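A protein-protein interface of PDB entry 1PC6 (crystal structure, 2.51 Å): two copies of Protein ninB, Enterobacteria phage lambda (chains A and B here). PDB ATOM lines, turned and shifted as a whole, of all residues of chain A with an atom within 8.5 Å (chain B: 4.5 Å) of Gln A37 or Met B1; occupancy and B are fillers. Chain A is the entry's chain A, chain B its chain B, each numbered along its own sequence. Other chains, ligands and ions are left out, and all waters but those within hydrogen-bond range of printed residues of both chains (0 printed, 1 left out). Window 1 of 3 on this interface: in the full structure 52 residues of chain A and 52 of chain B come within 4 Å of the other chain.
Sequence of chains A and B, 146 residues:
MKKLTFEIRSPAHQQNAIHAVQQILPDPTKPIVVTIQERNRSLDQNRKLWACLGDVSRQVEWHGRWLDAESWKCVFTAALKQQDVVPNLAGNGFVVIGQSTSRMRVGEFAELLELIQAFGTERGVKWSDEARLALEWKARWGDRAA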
ATOM      1  N   PHE A   6       5.661 -25.048 -26.601  1.00  0.00           N
ATOM      2  CA  PHE A   6       5.214 -23.691 -26.393  1.00  0.00           C
ATOM      3  C   PHE A   6       3.714 -23.640 -26.266  1.00  0.00           C
ATOM      4  O   PHE A   6       3.011 -23.412 -27.242  1.00  0.00           O
ATOM      5  CB  PHE A   6       5.625 -22.786 -27.556  1.00  0.00           C
ATOM      6  CG  PHE A   6       7.091 -22.806 -27.863  1.00  0.00           C
ATOM      7  CD1 PHE A   6       7.629 -23.789 -28.684  1.00  0.00           C
ATOM      8  CD2 PHE A   6       7.938 -21.836 -27.338  1.00  0.00           C
ATOM      9  CE1 PHE A   6       8.990 -23.804 -28.979  1.00  0.00           C
ATOM     10  CE2 PHE A   6       9.300 -21.843 -27.625  1.00  0.00           C
ATOM     11  CZ  PHE A   6       9.825 -22.828 -28.448  1.00  0.00           C
ATOM     12  N   GLU A   7       3.213 -23.876 -25.071  1.00  0.00           N
ATOM     13  CA  GLU A   7       1.783 -23.768 -24.876  1.00  0.00           C
ATOM     14  C   GLU A   7       1.505 -22.279 -25.071  1.00  0.00           C
ATOM     15  O   GLU A   7       2.075 -21.440 -24.373  1.00  0.00           O
ATOM     16  CB  GLU A   7       1.417 -24.194 -23.461  1.00  0.00           C
ATOM     17  CG  GLU A   7       0.197 -23.513 -22.900  1.00  0.00           C
ATOM     18  CD  GLU A   7      -0.076 -23.939 -21.477  1.00  0.00           C
ATOM     19  OE1 GLU A   7       0.878 -23.954 -20.665  1.00  0.00           O
ATOM     20  OE2 GLU A   7      -1.245 -24.254 -21.173  1.00  0.00           O
ATOM     21  N   ILE A   8       0.657 -21.945 -26.036  1.00  0.00           N
ATOM     22  CA  ILE A   8       0.350 -20.546 -26.284  1.00  0.00           C
ATOM     23  C   ILE A   8      -0.765 -20.072 -25.367  1.00  0.00           C
ATOM     24  O   ILE A   8      -1.923 -20.480 -25.499  1.00  0.00           O
ATOM     25  CB  ILE A   8      -0.052 -20.313 -27.740  1.00  0.00           C
ATOM     26  CG1 ILE A   8       1.109 -20.707 -28.651  1.00  0.00           C
ATOM     27  CG2 ILE A   8      -0.411 -18.857 -27.949  1.00  0.00           C
ATOM     28  CD1 ILE A   8       0.786 -20.617 -30.109  1.00  0.00           C
ATOM     29  N   VAL A  34       7.035 -29.976 -36.376  1.00  0.00           N
ATOM     30  CA  VAL A  34       6.425 -28.866 -35.654  1.00  0.00           C
ATOM     31  C   VAL A  34       4.946 -29.205 -35.613  1.00  0.00           C
ATOM     32  O   VAL A  34       4.215 -28.980 -36.571  1.00  0.00           O
ATOM     33  CB  VAL A  34       6.582 -27.529 -36.385  1.00  0.00           C
ATOM     34  CG1 VAL A  34       5.750 -26.469 -35.689  1.00  0.00           C
ATOM     35  CG2 VAL A  34       8.039 -27.119 -36.407  1.00  0.00           C
ATOM     36  N   THR A  35       4.504 -29.758 -34.499  1.00  0.00           N
ATOM     37  CA  THR A  35       3.117 -30.146 -34.377  1.00  0.00           C
ATOM     38  C   THR A  35       2.314 -29.213 -33.484  1.00  0.00           C
ATOM     39  O   THR A  35       2.650 -28.997 -32.321  1.00  0.00           O
ATOM     40  CB  THR A  35       3.029 -31.603 -33.865  1.00  0.00           C
ATOM     41  OG1 THR A  35       1.788 -31.807 -33.179  1.00  0.00           O
ATOM     42  CG2 THR A  35       4.210 -31.918 -32.941  1.00  0.00           C
ATOM     43  N   ILE A  36       1.259 -28.642 -34.058  1.00  0.00           N
ATOM     44  CA  ILE A  36       0.360 -27.743 -33.337  1.00  0.00           C
ATOM     45  C   ILE A  36      -0.797 -28.608 -32.824  1.00  0.00           C
ATOM     46  O   ILE A  36      -1.056 -29.684 -33.360  1.00  0.00           O
ATOM     47  CB  ILE A  36      -0.203 -26.657 -34.274  1.00  0.00           C
ATOM     48  CG1 ILE A  36       0.950 -25.913 -34.965  1.00  0.00           C
ATOM     49  CG2 ILE A  36      -1.087 -25.708 -33.482  1.00  0.00           C
ATOM     50  CD1 ILE A  36       0.522 -24.933 -36.062  1.00  0.00           C
ATOM     51  N   GLN A  37      -1.502 -28.162 -31.794  1.00  0.00           N
ATOM     52  CA  GLN A  37      -2.589 -28.981 -31.296  1.00  0.00           C
ATOM     53  C   GLN A  37      -3.622 -28.279 -30.420  1.00  0.00           C
ATOM     54  O   GLN A  37      -3.277 -27.555 -29.489  1.00  0.00           O
ATOM     55  CB  GLN A  37      -2.009 -30.181 -30.544  1.00  0.00           C
ATOM     56  CG  GLN A  37      -3.071 -31.074 -29.921  1.00  0.00           C
ATOM     57  CD  GLN A  37      -2.498 -32.335 -29.283  1.00  0.00           C
ATOM     58  OE1 GLN A  37      -2.085 -33.275 -29.982  1.00  0.00           O
ATOM     59  NE2 GLN A  37      -2.467 -32.362 -27.946  1.00  0.00           N
ATOM     60  N   GLU A  38      -4.895 -28.505 -30.736  1.00  0.00           N
ATOM     61  CA  GLU A  38      -6.012 -27.950 -29.972  1.00  0.00           C
ATOM     62  C   GLU A  38      -5.955 -28.508 -28.558  1.00  0.00           C
ATOM     63  O   GLU A  38      -5.397 -29.581 -28.322  1.00  0.00           O
ATOM     64  CB  GLU A  38      -7.343 -28.373 -30.594  1.00  0.00           C
ATOM     65  CG  GLU A  38      -7.815 -27.511 -31.732  1.00  0.00           C
ATOM     66  CD  GLU A  38      -8.330 -26.174 -31.250  1.00  0.00           C
ATOM     67  OE1 GLU A  38      -7.582 -25.479 -30.526  1.00  0.00           O
ATOM     68  OE2 GLU A  38      -9.482 -25.816 -31.593  1.00  0.00           O
ATOM     69  N   ARG A  39      -6.535 -27.787 -27.612  1.00  0.00           N
ATOM     70  CA  ARG A  39      -6.550 -28.270 -26.246  1.00  0.00           C
ATOM     71  C   ARG A  39      -7.772 -27.776 -25.510  1.00  0.00           C
ATOM     72  O   ARG A  39      -8.141 -26.606 -25.606  1.00  0.00           O
ATOM     73  CB  ARG A  39      -5.284 -27.849 -25.511  1.00  0.00           C
ATOM     74  CG  ARG A  39      -4.035 -28.541 -26.017  1.00  0.00           C
ATOM     75  CD  ARG A  39      -3.218 -29.076 -24.864  1.00  0.00           C
ATOM     76  NE  ARG A  39      -3.254 -30.534 -24.789  1.00  0.00           N
ATOM     77  CZ  ARG A  39      -2.712 -31.244 -23.800  1.00  0.00           C
ATOM     78  NH1 ARG A  39      -2.095 -30.628 -22.797  1.00  0.00           N
ATOM     79  NH2 ARG A  39      -2.773 -32.569 -23.814  1.00  0.00           N
ATOM     80  N   ASN A  40      -8.412 -28.691 -24.791  1.00  0.00           N
ATOM     81  CA  ASN A  40      -9.601 -28.364 -24.030  1.00  0.00           C
ATOM     82  C   ASN A  40      -9.214 -28.127 -22.582  1.00  0.00           C
ATOM     83  O   ASN A  40      -9.653 -27.159 -21.961  1.00  0.00           O
ATOM     84  CB  ASN A  40     -10.622 -29.494 -24.130  1.00  0.00           C
ATOM     85  CG  ASN A  40     -11.141 -29.684 -25.547  1.00  0.00           C
ATOM     86  OD1 ASN A  40     -12.138 -30.379 -25.767  1.00  0.00           O
ATOM     87  ND2 ASN A  40     -10.463 -29.074 -26.515  1.00  0.00           N
ATOM     88  N   ARG A  41      -8.387 -29.013 -22.043  1.00  0.00           N
ATOM     89  CA  ARG A  41      -7.935 -28.869 -20.669  1.00  0.00           C
ATOM     90  C   ARG A  41      -6.495 -28.350 -20.680  1.00  0.00           C
ATOM     91  O   ARG A  41      -5.621 -28.952 -21.303  1.00  0.00           O
ATOM     92  CB  ARG A  41      -8.019 -30.214 -19.948  1.00  0.00           C
ATOM     93  N   LEU A  43      -2.597 -27.226 -20.083  1.00  0.00           N
ATOM     94  CA  LEU A  43      -1.426 -28.096 -19.996  1.00  0.00           C
ATOM     95  C   LEU A  43      -1.044 -28.306 -18.532  1.00  0.00           C
ATOM     96  O   LEU A  43      -0.553 -29.368 -18.139  1.00  0.00           O
ATOM     97  CB  LEU A  43      -0.252 -27.450 -20.734  1.00  0.00           C
ATOM     98  CG  LEU A  43       0.988 -28.287 -21.016  1.00  0.00           C
ATOM     99  CD1 LEU A  43       0.650 -29.310 -22.079  1.00  0.00           C
ATOM    100  CD2 LEU A  43       2.119 -27.395 -21.485  1.00  0.00           C
ATOM    101  N   SER A 100     -14.275 -40.014 -22.970  1.00  0.00           N
ATOM    102  CA  SER A 100     -13.023 -39.316 -23.221  1.00  0.00           C
ATOM    103  C   SER A 100     -12.845 -38.113 -22.308  1.00  0.00           C
ATOM    104  O   SER A 100     -13.685 -37.208 -22.279  1.00  0.00           O
ATOM    105  CB  SER A 100     -12.968 -38.856 -24.679  1.00  0.00           C
ATOM    106  OG  SER A 100     -11.813 -38.070 -24.915  1.00  0.00           O
ATOM    107  N   SER A 102     -10.549 -36.006 -22.678  1.00  0.00           N
ATOM    108  CA  SER A 102     -10.179 -34.940 -23.607  1.00  0.00           C
ATOM    109  C   SER A 102     -11.429 -34.184 -24.057  1.00  0.00           C
ATOM    110  O   SER A 102     -11.483 -32.953 -23.998  1.00  0.00           O
ATOM    111  CB  SER A 102      -9.487 -35.529 -24.841  1.00  0.00           C
ATOM    112  OG  SER A 102      -8.395 -36.356 -24.469  1.00  0.00           O
ATOM    113  N   ARG A 103     -12.434 -34.930 -24.503  1.00  0.00           N
ATOM    114  CA  ARG A 103     -13.679 -34.340 -24.967  1.00  0.00           C
ATOM    115  C   ARG A 103     -14.429 -33.628 -23.844  1.00  0.00           C
ATOM    116  O   ARG A 103     -15.176 -32.692 -24.106  1.00  0.00           O
ATOM    117  CB  ARG A 103     -14.563 -35.417 -25.590  1.00  0.00           C
ATOM    118  N   MET B   1      -8.219 -36.308 -30.471  1.00  0.00           N
ATOM    119  CA  MET B   1      -7.141 -35.250 -30.664  1.00  0.00           C
ATOM    120  C   MET B   1      -7.570 -34.092 -31.633  1.00  0.00           C
ATOM    121  O   MET B   1      -8.808 -33.861 -31.868  1.00  0.00           O
ATOM    122  CB  MET B   1      -5.820 -35.948 -31.146  1.00  0.00           C
ATOM    123  CG  MET B   1      -5.261 -36.969 -30.086  1.00  0.00           C
ATOM    124  SD  MET B   1      -3.657 -37.802 -30.576  1.00  0.00           S
ATOM    125  CE  MET B   1      -2.396 -36.247 -30.609  1.00  0.00           C
ATOM    126  N   LYS B   2      -6.563 -33.381 -32.159  1.00  0.00           N
ATOM    127  CA  LYS B   2      -6.715 -32.249 -33.083  1.00  0.00           C
ATOM    128  C   LYS B   2      -5.301 -31.708 -33.288  1.00  0.00           C
ATOM    129  O   LYS B   2      -5.065 -30.520 -33.089  1.00  0.00           O
ATOM    130  CB  LYS B   2      -7.580 -31.137 -32.463  1.00  0.00           C
ATOM    131  CG  LYS B   2      -9.079 -31.265 -32.682  1.00  0.00           C
ATOM    132  CD  LYS B   2      -9.861 -30.388 -31.713  1.00  0.00           C
ATOM    133  CE  LYS B   2      -9.836 -30.960 -30.307  1.00  0.00           C
ATOM    134  NZ  LYS B   2     -10.410 -30.010 -29.315  1.00  0.00           N
ATOM    135  N   LYS B   3      -4.365 -32.575 -33.676  1.00  0.00           N
ATOM    136  CA  LYS B   3      -2.976 -32.156 -33.859  1.00  0.00           C
ATOM    137  C   LYS B   3      -2.451 -32.076 -35.294  1.00  0.00           C
ATOM    138  O   LYS B   3      -2.183 -33.093 -35.933  1.00  0.00           O
ATOM    139  CB  LYS B   3      -2.047 -33.054 -33.019  1.00  0.00           C
ATOM    140  CG  LYS B   3      -2.208 -34.579 -33.248  1.00  0.00           C
ATOM    141  CD  LYS B   3      -1.034 -35.218 -34.104  1.00  0.00           C
ATOM    142  CE  LYS B   3      -1.143 -36.796 -34.227  1.00  0.00           C
ATOM    143  NZ  LYS B   3      -1.235 -37.517 -32.864  1.00  0.00           N
ATOM    144  N   PRO B  31      -6.081 -23.182 -24.493  1.00  0.00           N
ATOM    145  CA  PRO B  31      -4.793 -23.003 -25.175  1.00  0.00           C
ATOM    146  C   PRO B  31      -4.536 -23.871 -26.408  1.00  0.00           C
ATOM    147  O   PRO B  31      -5.204 -24.881 -26.642  1.00  0.00           O
ATOM    148  CB  PRO B  31      -3.789 -23.295 -24.068  1.00  0.00           C
ATOM    149  CG  PRO B  31      -4.441 -24.465 -23.394  1.00  0.00           C
ATOM    150  CD  PRO B  31      -5.912 -24.035 -23.299  1.00  0.00           C
ATOM    151  N   ILE B  32      -3.551 -23.448 -27.190  1.00  0.00           N
ATOM    152  CA  ILE B  32      -3.134 -24.162 -28.384  1.00  0.00           C
ATOM    153  C   ILE B  32      -1.634 -24.379 -28.200  1.00  0.00           C
ATOM    154  O   ILE B  32      -0.864 -23.426 -28.194  1.00  0.00           O
ATOM    155  CB  ILE B  32      -3.404 -23.328 -29.646  1.00  0.00           C
ATOM    156  CG1 ILE B  32      -4.898 -23.019 -29.734  1.00  0.00           C
ATOM    157  CG2 ILE B  32      -2.920 -24.071 -30.876  1.00  0.00           C
ATOM    158  CD1 ILE B  32      -5.314 -22.272 -30.977  1.00  0.00           C
ATOM    159  N   VAL B  33      -1.230 -25.634 -28.019  1.00  0.00           N
ATOM    160  CA  VAL B  33       0.176 -25.969 -27.807  1.00  0.00           C
ATOM    161  C   VAL B  33       0.941 -26.303 -29.094  1.00  0.00           C
ATOM    162  O   VAL B  33       0.483 -27.090 -29.917  1.00  0.00           O
ATOM    163  CB  VAL B  33       0.304 -27.161 -26.825  1.00  0.00           C
ATOM    164  CG1 VAL B  33       1.759 -27.553 -26.659  1.00  0.00           C
ATOM    165  CG2 VAL B  33      -0.287 -26.785 -25.477  1.00  0.00           C
ATOM    166  N   TRP B  50      -3.195 -42.368 -34.930  1.00  0.00           N
ATOM    167  CA  TRP B  50      -4.258 -41.391 -34.844  1.00  0.00           C
ATOM    168  C   TRP B  50      -4.752 -40.913 -36.196  1.00  0.00           C
ATOM    169  O   TRP B  50      -5.896 -40.487 -36.317  1.00  0.00           O
ATOM    170  CB  TRP B  50      -3.800 -40.212 -33.988  1.00  0.00           C
ATOM    171  CG  TRP B  50      -3.669 -40.605 -32.565  1.00  0.00           C
ATOM    172  CD1 TRP B  50      -2.519 -40.740 -31.849  1.00  0.00           C
ATOM    173  CD2 TRP B  50      -4.733 -40.991 -31.694  1.00  0.00           C
ATOM    174  NE1 TRP B  50      -2.800 -41.192 -30.581  1.00  0.00           N
ATOM    175  CE2 TRP B  50      -4.154 -41.353 -30.461  1.00  0.00           C
ATOM    176  CE3 TRP B  50      -6.123 -41.071 -31.838  1.00  0.00           C
ATOM    177  CZ2 TRP B  50      -4.918 -41.786 -29.378  1.00  0.00           C
ATOM    178  CZ3 TRP B  50      -6.878 -41.502 -30.764  1.00  0.00           C
ATOM    179  CH2 TRP B  50      -6.274 -41.854 -29.547  1.00  0.00           C
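The backbone NH (N) of Arg A39 lies close to the backbone carbonyl oxygen (O) of Pro B31 (3.3 Å).
N of Glu A38 sits at hydrogen-bond distance from O of Lys B2 (3.1 Å).
The backbone NH (N) of Ile A8 lies within hydrogen-bond range of the backbone carbonyl oxygen (O) of Ile B32 (3.0 Å).
N of Gln A37 lies within hydrogen-bond range of O of Val B33 (2.9 Å).
The side-chain amide nitrogen of Asn A40 sits close to the side-chain amino group of Lys B2, 3.0 Å away.
NE1 of Trp B50 lies close to SD of Met B1, 3.5 Å away.
The side-chain sulfur of Met B1 lies close to the side-chain amino group of Lys B3, 3.3 Å away.
The side-chain amide oxygen (OD1) of Asn A40 sits close to the backbone carbonyl oxygen (O) of Ser A102, at 3.2 Å.
The side-chain carboxylate (OE2) of Glu A7 lies close to the backbone NH (N) of Leu A43, at 3.4 Å.
O of Phe A6 touches O of Ile B32 (3.99 Å).
Glu A7 touches Pro B31.
CG2 of Val B33 touches CB of Glu A7, at 3.7 Å.
Ile A8 touches Pro B31.
O of Thr A35 touches O of Val B33, at 3.8 Å.
O of Val B33 touches CA of Ile A36, 3.5 Å away.
Gln A37 touches Met B1 (OE1 to CE, 3.1 Å).
Gln A37 touches Lys B3.
O of Gln A37 touches CA of Ile B32, 3.6 Å away.
Arg A39 touches Val B33.
Printed residues of chain B within 4 Å of Gln A37: Met B1 (3.1 Å), Lys B2 (3.4 Å), Lys B3 (3.0 Å), Ile B32 (3.6 Å) and Val B33 (2.9 Å).
Met B1 touches just one residue of chain A: Gln A37 (3.1 Å).
Printed residues of chain A within 4 Å of Pro B31: Glu A7, Ile A8 and Arg A39.
Printed residues of chain B within 4 Å of Ile A8: Pro B31 (3.7 Å) and Ile B32 (3.0 Å).
Printed residues of chain B within 4 Å of Phe A6: Ile B32 (3.99 Å) and Val B33 (3.9 Å).
Of the printed residues of chain A, Val B33 touches Phe A6, Glu A7, Thr A35, Ile A36, Gln A37 and Arg A39.
Val A34 touches none of the printed residues of chain B.
Printed residues of chain B that touch a printed residue of chain A: Met B1, Lys B2, Lys B3, Pro B31, Ile B32 and Val B33.
Hydrophobic or aromatic side chains of chain B within 4 Å of the printed part of chain A: Met B1, Pro B31, Ile B32 and Val B33.
Of the 15 printed residues of chain A, 9 touch a printed residue of chain B.
Hydrophobic or aromatic side chains of chain A that line the printed part of chain B: Ile A8 and Ile A36.
Among the printed residues, 20 pairs touch across the chains.
Among the printed residues, no Asp or Glu carboxylate lies within 4 Å of a Lys or Arg side-chain nitrogen of the other chain.
No position is printed for both chains.
Of the 20 pairs that touch across the chains among the printed residues, none has its exchanged pair printed and touching as well.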
